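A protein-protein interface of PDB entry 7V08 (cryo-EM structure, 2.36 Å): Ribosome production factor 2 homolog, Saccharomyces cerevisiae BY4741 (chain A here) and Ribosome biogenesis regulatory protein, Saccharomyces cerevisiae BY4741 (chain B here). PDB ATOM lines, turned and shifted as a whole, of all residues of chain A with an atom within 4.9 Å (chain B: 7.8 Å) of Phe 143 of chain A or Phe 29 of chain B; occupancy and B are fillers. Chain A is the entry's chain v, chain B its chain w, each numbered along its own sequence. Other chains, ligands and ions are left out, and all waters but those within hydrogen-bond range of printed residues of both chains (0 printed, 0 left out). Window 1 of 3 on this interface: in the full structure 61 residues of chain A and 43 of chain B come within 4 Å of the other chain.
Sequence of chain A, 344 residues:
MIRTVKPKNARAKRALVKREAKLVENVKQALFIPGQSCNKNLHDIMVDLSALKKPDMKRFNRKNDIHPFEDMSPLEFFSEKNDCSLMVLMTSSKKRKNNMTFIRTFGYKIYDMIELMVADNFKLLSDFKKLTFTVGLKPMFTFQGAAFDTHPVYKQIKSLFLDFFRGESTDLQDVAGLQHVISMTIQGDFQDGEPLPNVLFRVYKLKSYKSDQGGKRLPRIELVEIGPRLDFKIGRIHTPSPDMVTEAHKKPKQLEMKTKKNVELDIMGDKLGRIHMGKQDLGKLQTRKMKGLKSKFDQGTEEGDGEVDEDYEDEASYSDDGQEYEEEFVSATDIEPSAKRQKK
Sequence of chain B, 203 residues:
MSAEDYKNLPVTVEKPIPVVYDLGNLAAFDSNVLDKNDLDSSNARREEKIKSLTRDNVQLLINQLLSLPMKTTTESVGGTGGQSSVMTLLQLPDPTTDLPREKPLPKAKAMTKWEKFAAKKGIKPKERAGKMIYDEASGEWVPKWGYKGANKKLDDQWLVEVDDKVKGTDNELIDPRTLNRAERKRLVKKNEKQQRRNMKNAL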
ATOM      1  N   PHE A 141       0.244  24.829   9.778  1.00  0.00           N
ATOM      2  CA  PHE A 141       0.347  26.130  10.423  1.00  0.00           C
ATOM      3  C   PHE A 141       1.784  26.616  10.390  1.00  0.00           C
ATOM      4  O   PHE A 141       2.720  25.821  10.504  1.00  0.00           O
ATOM      5  CB  PHE A 141      -0.127  26.087  11.875  1.00  0.00           C
ATOM      6  CG  PHE A 141      -1.586  25.803  12.031  1.00  0.00           C
ATOM      7  CD1 PHE A 141      -2.513  26.831  12.000  1.00  0.00           C
ATOM      8  CD2 PHE A 141      -2.033  24.510  12.220  1.00  0.00           C
ATOM      9  CE1 PHE A 141      -3.855  26.570  12.149  1.00  0.00           C
ATOM     10  CE2 PHE A 141      -3.376  24.243  12.371  1.00  0.00           C
ATOM     11  CZ  PHE A 141      -4.288  25.275  12.339  1.00  0.00           C
ATOM     12  N   THR A 142       1.948  27.928  10.232  1.00  0.00           N
ATOM     13  CA  THR A 142       3.235  28.592  10.406  1.00  0.00           C
ATOM     14  C   THR A 142       3.030  29.863  11.216  1.00  0.00           C
ATOM     15  O   THR A 142       2.069  30.604  10.982  1.00  0.00           O
ATOM     16  CB  THR A 142       3.890  28.921   9.065  1.00  0.00           C
ATOM     17  OG1 THR A 142       2.895  29.407   8.160  1.00  0.00           O
ATOM     18  CG2 THR A 142       4.559  27.681   8.477  1.00  0.00           C
ATOM     19  N   PHE A 143       3.921  30.102  12.175  1.00  0.00           N
ATOM     20  CA  PHE A 143       3.830  31.248  13.071  1.00  0.00           C
ATOM     21  C   PHE A 143       5.165  31.974  13.067  1.00  0.00           C
ATOM     22  O   PHE A 143       6.132  31.497  13.668  1.00  0.00           O
ATOM     23  CB  PHE A 143       3.467  30.812  14.492  1.00  0.00           C
ATOM     24  CG  PHE A 143       2.031  30.439  14.663  1.00  0.00           C
ATOM     25  CD1 PHE A 143       1.590  29.169  14.341  1.00  0.00           C
ATOM     26  CD2 PHE A 143       1.118  31.356  15.148  1.00  0.00           C
ATOM     27  CE1 PHE A 143       0.269  28.822  14.497  1.00  0.00           C
ATOM     28  CE2 PHE A 143      -0.206  31.013  15.307  1.00  0.00           C
ATOM     29  CZ  PHE A 143      -0.629  29.746  14.979  1.00  0.00           C
ATOM     30  N   GLN A 144       5.207  33.133  12.418  1.00  0.00           N
ATOM     31  CA  GLN A 144       6.429  33.914  12.274  1.00  0.00           C
ATOM     32  C   GLN A 144       6.445  35.013  13.328  1.00  0.00           C
ATOM     33  O   GLN A 144       5.564  35.885  13.341  1.00  0.00           O
ATOM     34  CB  GLN A 144       6.540  34.515  10.873  1.00  0.00           C
ATOM     35  CG  GLN A 144       6.934  33.533   9.780  1.00  0.00           C
ATOM     36  CD  GLN A 144       5.774  32.686   9.298  1.00  0.00           C
ATOM     37  OE1 GLN A 144       4.621  32.938   9.642  1.00  0.00           O
ATOM     38  NE2 GLN A 144       6.077  31.672   8.496  1.00  0.00           N
ATOM     39  N   GLY A 145       7.445  34.966  14.208  1.00  0.00           N
ATOM     40  CA  GLY A 145       7.600  35.952  15.258  1.00  0.00           C
ATOM     41  C   GLY A 145       7.857  35.362  16.632  1.00  0.00           C
ATOM     42  O   GLY A 145       7.148  34.449  17.064  1.00  0.00           O
ATOM     43  N   PHE A 148       5.048  35.258  19.496  1.00  0.00           N
ATOM     44  CA  PHE A 148       4.133  34.125  19.595  1.00  0.00           C
ATOM     45  C   PHE A 148       4.563  33.145  20.677  1.00  0.00           C
ATOM     46  O   PHE A 148       3.716  32.495  21.297  1.00  0.00           O
ATOM     47  CB  PHE A 148       4.039  33.409  18.249  1.00  0.00           C
ATOM     48  CG  PHE A 148       3.151  34.096  17.263  1.00  0.00           C
ATOM     49  CD1 PHE A 148       1.911  34.572  17.647  1.00  0.00           C
ATOM     50  CD2 PHE A 148       3.555  34.269  15.954  1.00  0.00           C
ATOM     51  CE1 PHE A 148       1.088  35.203  16.741  1.00  0.00           C
ATOM     52  CE2 PHE A 148       2.740  34.906  15.049  1.00  0.00           C
ATOM     53  CZ  PHE A 148       1.508  35.374  15.441  1.00  0.00           C
ATOM     54  N   LYS A 158      -1.868  32.754  19.204  1.00  0.00           N
ATOM     55  CA  LYS A 158      -1.422  31.485  18.637  1.00  0.00           C
ATOM     56  C   LYS A 158      -2.264  30.324  19.146  1.00  0.00           C
ATOM     57  O   LYS A 158      -2.704  29.477  18.357  1.00  0.00           O
ATOM     58  CB  LYS A 158       0.050  31.251  18.968  1.00  0.00           C
ATOM     59  CG  LYS A 158       0.527  29.853  18.638  1.00  0.00           C
ATOM     60  CD  LYS A 158       1.964  29.618  19.052  1.00  0.00           C
ATOM     61  CE  LYS A 158       2.100  29.512  20.555  1.00  0.00           C
ATOM     62  NZ  LYS A 158       3.455  29.055  20.960  1.00  0.00           N
ATOM     63  N   PHE A 161      -5.813  30.419  17.560  1.00  0.00           N
ATOM     64  CA  PHE A 161      -5.956  30.072  16.151  1.00  0.00           C
ATOM     65  C   PHE A 161      -5.616  28.609  15.898  1.00  0.00           C
ATOM     66  O   PHE A 161      -6.247  27.964  15.045  1.00  0.00           O
ATOM     67  CB  PHE A 161      -5.126  31.017  15.291  1.00  0.00           C
ATOM     68  CG  PHE A 161      -5.815  32.328  15.035  1.00  0.00           C
ATOM     69  CD1 PHE A 161      -6.718  32.456  13.994  1.00  0.00           C
ATOM     70  CD2 PHE A 161      -5.604  33.411  15.864  1.00  0.00           C
ATOM     71  CE1 PHE A 161      -7.368  33.652  13.766  1.00  0.00           C
ATOM     72  CE2 PHE A 161      -6.250  34.612  15.642  1.00  0.00           C
ATOM     73  CZ  PHE A 161      -7.135  34.732  14.593  1.00  0.00           C
ATOM     74  N   LEU A 162      -4.653  28.054  16.645  1.00  0.00           N
ATOM     75  CA  LEU A 162      -4.427  26.614  16.585  1.00  0.00           C
ATOM     76  C   LEU A 162      -5.676  25.853  16.993  1.00  0.00           C
ATOM     77  O   LEU A 162      -6.093  24.917  16.302  1.00  0.00           O
ATOM     78  CB  LEU A 162      -3.257  26.216  17.483  1.00  0.00           C
ATOM     79  CG  LEU A 162      -1.847  26.464  16.966  1.00  0.00           C
ATOM     80  CD1 LEU A 162      -0.842  26.240  18.082  1.00  0.00           C
ATOM     81  CD2 LEU A 162      -1.554  25.562  15.794  1.00  0.00           C
ATOM     82  N   MET A 184       0.396  32.883  10.256  1.00  0.00           N
ATOM     83  CA  MET A 184       0.214  34.053  11.105  1.00  0.00           C
ATOM     84  C   MET A 184       1.598  34.641  11.332  1.00  0.00           C
ATOM     85  O   MET A 184       2.468  33.983  11.912  1.00  0.00           O
ATOM     86  CB  MET A 184      -0.454  33.687  12.427  1.00  0.00           C
ATOM     87  CG  MET A 184      -1.698  32.826  12.286  1.00  0.00           C
ATOM     88  SD  MET A 184      -3.202  33.802  12.164  1.00  0.00           S
ATOM     89  CE  MET A 184      -3.115  34.713  13.698  1.00  0.00           C
ATOM     90  N   ILE B  17      18.241  31.057  13.780  1.00  0.00           N
ATOM     91  CA  ILE B  17      17.594  30.385  14.906  1.00  0.00           C
ATOM     92  C   ILE B  17      16.785  29.212  14.367  1.00  0.00           C
ATOM     93  O   ILE B  17      15.955  29.398  13.465  1.00  0.00           O
ATOM     94  CB  ILE B  17      16.709  31.350  15.710  1.00  0.00           C
ATOM     95  CG1 ILE B  17      17.559  32.434  16.378  1.00  0.00           C
ATOM     96  CG2 ILE B  17      15.877  30.592  16.734  1.00  0.00           C
ATOM     97  CD1 ILE B  17      17.590  33.729  15.609  1.00  0.00           C
ATOM     98  N   PRO B  18      16.998  27.996  14.873  1.00  0.00           N
ATOM     99  CA  PRO B  18      16.280  26.830  14.336  1.00  0.00           C
ATOM    100  C   PRO B  18      14.778  26.924  14.570  1.00  0.00           C
ATOM    101  O   PRO B  18      14.322  27.395  15.613  1.00  0.00           O
ATOM    102  CB  PRO B  18      16.895  25.652  15.099  1.00  0.00           C
ATOM    103  CG  PRO B  18      17.441  26.258  16.353  1.00  0.00           C
ATOM    104  CD  PRO B  18      17.902  27.632  15.977  1.00  0.00           C
ATOM    105  N   VAL B  19      14.016  26.460  13.579  1.00  0.00           N
ATOM    106  CA  VAL B  19      12.569  26.368  13.707  1.00  0.00           C
ATOM    107  C   VAL B  19      12.221  25.200  14.618  1.00  0.00           C
ATOM    108  O   VAL B  19      12.806  24.115  14.515  1.00  0.00           O
ATOM    109  CB  VAL B  19      11.923  26.204  12.320  1.00  0.00           C
ATOM    110  CG1 VAL B  19      10.413  26.087  12.439  1.00  0.00           C
ATOM    111  CG2 VAL B  19      12.299  27.365  11.417  1.00  0.00           C
ATOM    112  N   VAL B  20      11.285  25.422  15.537  1.00  0.00           N
ATOM    113  CA  VAL B  20      10.777  24.348  16.380  1.00  0.00           C
ATOM    114  C   VAL B  20       9.488  23.824  15.765  1.00  0.00           C
ATOM    115  O   VAL B  20       8.776  24.542  15.054  1.00  0.00           O
ATOM    116  CB  VAL B  20      10.567  24.812  17.836  1.00  0.00           C
ATOM    117  CG1 VAL B  20      11.890  25.276  18.431  1.00  0.00           C
ATOM    118  CG2 VAL B  20       9.551  25.920  17.891  1.00  0.00           C
ATOM    119  N   TYR B  21       9.188  22.555  16.023  1.00  0.00           N
ATOM    120  CA  TYR B  21       8.113  21.866  15.327  1.00  0.00           C
ATOM    121  C   TYR B  21       7.138  21.235  16.308  1.00  0.00           C
ATOM    122  O   TYR B  21       7.537  20.719  17.355  1.00  0.00           O
ATOM    123  CB  TYR B  21       8.649  20.768  14.414  1.00  0.00           C
ATOM    124  CG  TYR B  21       9.634  21.235  13.381  1.00  0.00           C
ATOM    125  CD1 TYR B  21       9.215  21.946  12.267  1.00  0.00           C
ATOM    126  CD2 TYR B  21      10.981  20.946  13.508  1.00  0.00           C
ATOM    127  CE1 TYR B  21      10.115  22.364  11.318  1.00  0.00           C
ATOM    128  CE2 TYR B  21      11.884  21.355  12.566  1.00  0.00           C
ATOM    129  CZ  TYR B  21      11.450  22.063  11.473  1.00  0.00           C
ATOM    130  OH  TYR B  21      12.361  22.471  10.535  1.00  0.00           O
ATOM    131  N   ASP B  22       5.861  21.263  15.944  1.00  0.00           N
ATOM    132  CA  ASP B  22       4.811  20.489  16.592  1.00  0.00           C
ATOM    133  C   ASP B  22       4.167  19.673  15.476  1.00  0.00           C
ATOM    134  O   ASP B  22       3.213  20.121  14.834  1.00  0.00           O
ATOM    135  CB  ASP B  22       3.810  21.386  17.303  1.00  0.00           C
ATOM    136  CG  ASP B  22       2.747  20.601  18.032  1.00  0.00           C
ATOM    137  OD1 ASP B  22       2.978  19.406  18.307  1.00  0.00           O
ATOM    138  OD2 ASP B  22       1.677  21.171  18.322  1.00  0.00           O
ATOM    139  N   LEU B  23       4.714  18.484  15.226  1.00  0.00           N
ATOM    140  CA  LEU B  23       4.250  17.648  14.128  1.00  0.00           C
ATOM    141  C   LEU B  23       2.902  16.995  14.405  1.00  0.00           C
ATOM    142  O   LEU B  23       2.283  16.470  13.475  1.00  0.00           O
ATOM    143  CB  LEU B  23       5.294  16.576  13.814  1.00  0.00           C
ATOM    144  CG  LEU B  23       6.657  17.075  13.330  1.00  0.00           C
ATOM    145  CD1 LEU B  23       7.622  15.914  13.142  1.00  0.00           C
ATOM    146  CD2 LEU B  23       6.524  17.874  12.041  1.00  0.00           C
ATOM    147  N   ASN B  25       0.228  18.760  15.525  1.00  0.00           N
ATOM    148  CA  ASN B  25      -0.698  19.748  14.995  1.00  0.00           C
ATOM    149  C   ASN B  25      -0.271  20.288  13.637  1.00  0.00           C
ATOM    150  O   ASN B  25      -0.954  21.161  13.095  1.00  0.00           O
ATOM    151  CB  ASN B  25      -0.861  20.898  15.992  1.00  0.00           C
ATOM    152  CG  ASN B  25      -1.594  20.474  17.253  1.00  0.00           C
ATOM    153  OD1 ASN B  25      -2.379  19.527  17.237  1.00  0.00           O
ATOM    154  ND2 ASN B  25      -1.343  21.174  18.350  1.00  0.00           N
ATOM    155  N   LEU B  26       0.828  19.773  13.077  1.00  0.00           N
ATOM    156  CA  LEU B  26       1.395  20.228  11.801  1.00  0.00           C
ATOM    157  C   LEU B  26       1.732  21.718  11.832  1.00  0.00           C
ATOM    158  O   LEU B  26       1.336  22.481  10.949  1.00  0.00           O
ATOM    159  CB  LEU B  26       0.470  19.910  10.622  1.00  0.00           C
ATOM    160  CG  LEU B  26      -0.219  18.547  10.525  1.00  0.00           C
ATOM    161  CD1 LEU B  26      -1.282  18.598   9.448  1.00  0.00           C
ATOM    162  CD2 LEU B  26       0.768  17.430  10.234  1.00  0.00           C
ATOM    163  N   ALA B  27       2.474  22.140  12.852  1.00  0.00           N
ATOM    164  CA  ALA B  27       2.832  23.540  13.021  1.00  0.00           C
ATOM    165  C   ALA B  27       4.343  23.700  13.128  1.00  0.00           C
ATOM    166  O   ALA B  27       5.041  22.833  13.659  1.00  0.00           O
ATOM    167  CB  ALA B  27       2.162  24.138  14.261  1.00  0.00           C
ATOM    168  N   ALA B  28       4.839  24.824  12.616  1.00  0.00           N
ATOM    169  CA  ALA B  28       6.242  25.195  12.730  1.00  0.00           C
ATOM    170  C   ALA B  28       6.339  26.620  13.255  1.00  0.00           C
ATOM    171  O   ALA B  28       5.620  27.509  12.792  1.00  0.00           O
ATOM    172  CB  ALA B  28       6.966  25.080  11.385  1.00  0.00           C
ATOM    173  N   PHE B  29       7.223  26.833  14.227  1.00  0.00           N
ATOM    174  CA  PHE B  29       7.404  28.142  14.844  1.00  0.00           C
ATOM    175  C   PHE B  29       8.836  28.597  14.624  1.00  0.00           C
ATOM    176  O   PHE B  29       9.779  27.910  15.032  1.00  0.00           O
ATOM    177  CB  PHE B  29       7.088  28.104  16.340  1.00  0.00           C
ATOM    178  CG  PHE B  29       5.816  27.391  16.676  1.00  0.00           C
ATOM    179  CD1 PHE B  29       4.603  27.855  16.203  1.00  0.00           C
ATOM    180  CD2 PHE B  29       5.829  26.263  17.476  1.00  0.00           C
ATOM    181  CE1 PHE B  29       3.428  27.202  16.514  1.00  0.00           C
ATOM    182  CE2 PHE B  29       4.655  25.606  17.790  1.00  0.00           C
ATOM    183  CZ  PHE B  29       3.455  26.076  17.307  1.00  0.00           C
ATOM    184  N   ASP B  30       8.992  29.754  13.989  1.00  0.00           N
ATOM    185  CA  ASP B  30      10.287  30.392  13.806  1.00  0.00           C
ATOM    186  C   ASP B  30      10.272  31.741  14.511  1.00  0.00           C
ATOM    187  O   ASP B  30       9.377  32.558  14.279  1.00  0.00           O
ATOM    188  CB  ASP B  30      10.616  30.561  12.326  1.00  0.00           C
ATOM    189  CG  ASP B  30       9.469  31.151  11.539  1.00  0.00           C
ATOM    190  OD1 ASP B  30       8.327  30.686  11.719  1.00  0.00           O
ATOM    191  OD2 ASP B  30       9.713  32.082  10.745  1.00  0.00           O
ATOM    192  N   SER B  31      11.265  31.963  15.367  1.00  0.00           N
ATOM    193  CA  SER B  31      11.347  33.152  16.206  1.00  0.00           C
ATOM    194  C   SER B  31      12.477  34.081  15.771  1.00  0.00           C
ATOM    195  O   SER B  31      13.154  34.679  16.608  1.00  0.00           O
ATOM    196  CB  SER B  31      11.532  32.743  17.665  1.00  0.00           C
ATOM    197  OG  SER B  31      12.703  31.964  17.822  1.00  0.00           O
ATOM    198  N   ASN B  32      12.699  34.202  14.467  1.00  0.00           N
ATOM    199  CA  ASN B  32      13.821  34.993  13.985  1.00  0.00           C
ATOM    200  C   ASN B  32      13.466  36.478  13.952  1.00  0.00           C
ATOM    201  O   ASN B  32      12.340  36.890  14.239  1.00  0.00           O
ATOM    202  CB  ASN B  32      14.259  34.506  12.609  1.00  0.00           C
ATOM    203  CG  ASN B  32      15.038  33.212  12.682  1.00  0.00           C
ATOM    204  OD1 ASN B  32      16.262  33.208  12.588  1.00  0.00           O
ATOM    205  ND2 ASN B  32      14.332  32.105  12.874  1.00  0.00           N
ATOM    206  N   LEU B  34      12.337  39.782  12.599  1.00  0.00           N
ATOM    207  CA  LEU B  34      11.454  40.260  11.542  1.00  0.00           C
ATOM    208  C   LEU B  34      11.515  41.781  11.490  1.00  0.00           C
ATOM    209  O   LEU B  34      11.212  42.450  12.482  1.00  0.00           O
ATOM    210  CB  LEU B  34      10.016  39.792  11.780  1.00  0.00           C
ATOM    211  CG  LEU B  34       9.676  38.340  11.427  1.00  0.00           C
ATOM    212  CD1 LEU B  34       8.309  37.970  11.950  1.00  0.00           C
ATOM    213  CD2 LEU B  34       9.739  38.134   9.933  1.00  0.00           C
ATOM    214  N   THR B  54       7.092  32.174   4.530  1.00  0.00           N
ATOM    215  CA  THR B  54       6.163  31.059   4.685  1.00  0.00           C
ATOM    216  C   THR B  54       6.614  29.853   3.876  1.00  0.00           C
ATOM    217  O   THR B  54       6.475  28.712   4.323  1.00  0.00           O
ATOM    218  CB  THR B  54       4.754  31.464   4.258  1.00  0.00           C
ATOM    219  OG1 THR B  54       4.459  32.783   4.730  1.00  0.00           O
ATOM    220  CG2 THR B  54       3.743  30.488   4.834  1.00  0.00           C
ATOM    221  N   ASN B  57       9.463  28.149   5.822  1.00  0.00           N
ATOM    222  CA  ASN B  57       8.980  27.415   6.988  1.00  0.00           C
ATOM    223  C   ASN B  57       8.203  26.166   6.582  1.00  0.00           C
ATOM    224  O   ASN B  57       8.360  25.101   7.196  1.00  0.00           O
ATOM    225  CB  ASN B  57       8.132  28.334   7.868  1.00  0.00           C
ATOM    226  CG  ASN B  57       8.948  29.441   8.496  1.00  0.00           C
ATOM    227  OD1 ASN B  57       8.596  30.618   8.408  1.00  0.00           O
ATOM    228  ND2 ASN B  57      10.055  29.073   9.121  1.00  0.00           N
ATOM    229  N   LEU B  61       8.985  22.225   7.389  1.00  0.00           N
ATOM    230  CA  LEU B  61       7.943  21.381   7.964  1.00  0.00           C
ATOM    231  C   LEU B  61       7.709  20.133   7.119  1.00  0.00           C
ATOM    232  O   LEU B  61       7.562  19.029   7.655  1.00  0.00           O
ATOM    233  CB  LEU B  61       6.658  22.191   8.114  1.00  0.00           C
ATOM    234  CG  LEU B  61       5.441  21.492   8.715  1.00  0.00           C
ATOM    235  CD1 LEU B  61       5.608  21.309  10.212  1.00  0.00           C
ATOM    236  CD2 LEU B  61       4.185  22.273   8.395  1.00  0.00           C
ATOM    237  N   THR B  96       2.643  18.614  20.781  1.00  0.00           N
ATOM    238  CA  THR B  96       3.457  19.216  21.828  1.00  0.00           C
ATOM    239  C   THR B  96       2.763  20.413  22.461  1.00  0.00           C
ATOM    240  O   THR B  96       2.804  20.574  23.686  1.00  0.00           O
ATOM    241  CB  THR B  96       4.818  19.617  21.247  1.00  0.00           C
ATOM    242  OG1 THR B  96       5.603  18.441  21.018  1.00  0.00           O
ATOM    243  CG2 THR B  96       5.577  20.554  22.176  1.00  0.00           C
ATOM    244  N   THR B  97       2.093  21.229  21.653  1.00  0.00           N
ATOM    245  CA  THR B  97       1.454  22.438  22.155  1.00  0.00           C
ATOM    246  C   THR B  97       0.260  22.085  23.030  1.00  0.00           C
ATOM    247  O   THR B  97      -0.577  21.257  22.657  1.00  0.00           O
ATOM    248  CB  THR B  97       1.005  23.319  20.991  1.00  0.00           C
ATOM    249  OG1 THR B  97       0.088  22.590  20.163  1.00  0.00           O
ATOM    250  CG2 THR B  97       2.193  23.739  20.162  1.00  0.00           C
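The backbone NH (N) of Met 184 of chain A lies within hydrogen-bond range of the backbone carbonyl oxygen (O) of Thr 142 of chain A (2.9 Å).
N of Gln 144 of chain A sits at hydrogen-bond distance from O of Met 184 of chain A (2.9 Å).
The side-chain amino group of Lys 158 of chain A is in hydrogen-bond range of the backbone carbonyl oxygen of Phe 148 of chain A (3.5 Å).
The backbone carbonyl oxygen (O) of Val 20 of chain B lies within hydrogen-bond range of the backbone NH (N) of Phe 29 of chain B, at 2.9 Å.
The side-chain carboxylate (OD2) of Asp 22 of chain B sits at hydrogen-bond distance from the side-chain amide nitrogen (ND2) of Asn 25 of chain B (3.0 Å).
The side-chain hydroxyl (OG1) of Thr 97 of chain B sits at hydrogen-bond distance from the side-chain amide nitrogen (ND2) of Asn 25 of chain B, at 2.7 Å.
Phe 29 of chain B touches just these residues of chain A: Phe 143 and Lys 158.
Printed residues of chain A within 4 Å of Ala 27 of chain B: Phe 141.
Of the printed residues of chain A, Asn 25 of chain B touches Phe 141 (3.6 Å).
Phe 141 of chain A touches Ala 27 of chain B (O to CA, 3.4 Å).
Thr 142 of chain A touches Ala 28 of chain B.
OG1 of Thr 142 of chain A touches CG2 of Thr 54 of chain B, 3.6 Å away.
CG2 of Thr 142 of chain A touches CB of Asn 57 of chain B, at 3.7 Å.
Phe 143 of chain A touches Phe 29 of chain B.
Gln 144 of chain A touches Asp 30 of chain B (CG to OD2, 3.3 Å).
Gln 144 of chain A touches Leu 34 of chain B (O to CD1, 3.7 Å).
Gln 144 of chain A touches Thr 54 of chain B (NE2 to CA, 3.9 Å).
Gly 145 of chain A touches Leu 34 of chain B (N to CD1, 3.9 Å).
Phe 29 of chain B touches Lys 158 of chain A (CE1 to CD, 3.8 Å).
The backbone NH of Phe 141 of chain A is in hydrogen-bond range of the backbone carbonyl oxygen of Leu 26 of chain B, at 2.8 Å.
The backbone carbonyl oxygen (O) of Phe 141 of chain A sits at hydrogen-bond distance from the backbone NH (N) of Ala 28 of chain B, at 3.2 Å.
The backbone NH (N) of Phe 143 of chain A is in hydrogen-bond range of the backbone carbonyl oxygen (O) of Ala 28 of chain B (3.2 Å).
O of Phe 143 of chain A lies within hydrogen-bond range of N of Asp 30 of chain B.
The side-chain amide nitrogen of Gln 144 of chain A sits at hydrogen-bond distance from the side-chain amide oxygen of Asn 57 of chain B (2.7 Å).
The backbone NH of Gly 145 of chain A is in hydrogen-bond range of the backbone carbonyl oxygen of Asp 30 of chain B, at 3.1 Å.
Of the 21 printed residues of chain B, 9 touch a printed residue of chain A.
Hydrophobic or aromatic side chains of chain B within 4 Å of the printed part of chain A: Ala 27, Phe 29 and Leu 34.
Of the 10 printed residues of chain A, 6 touch a printed residue of chain B.
Printed residues of chain A that touch a printed residue of chain B: Phe 141, Thr 142, Phe 143, Gln 144, Gly 145 and Lys 158.
Hydrophobic or aromatic side chains of chain A within 4 Å of the printed part of chain B: Phe 141 and Phe 143.
Among the printed residues, 17 pairs touch across the chains.
Among the printed residues, no Asp or Glu carboxylate lies within 4 Å of a Lys or Arg side-chain nitrogen of the other chain.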
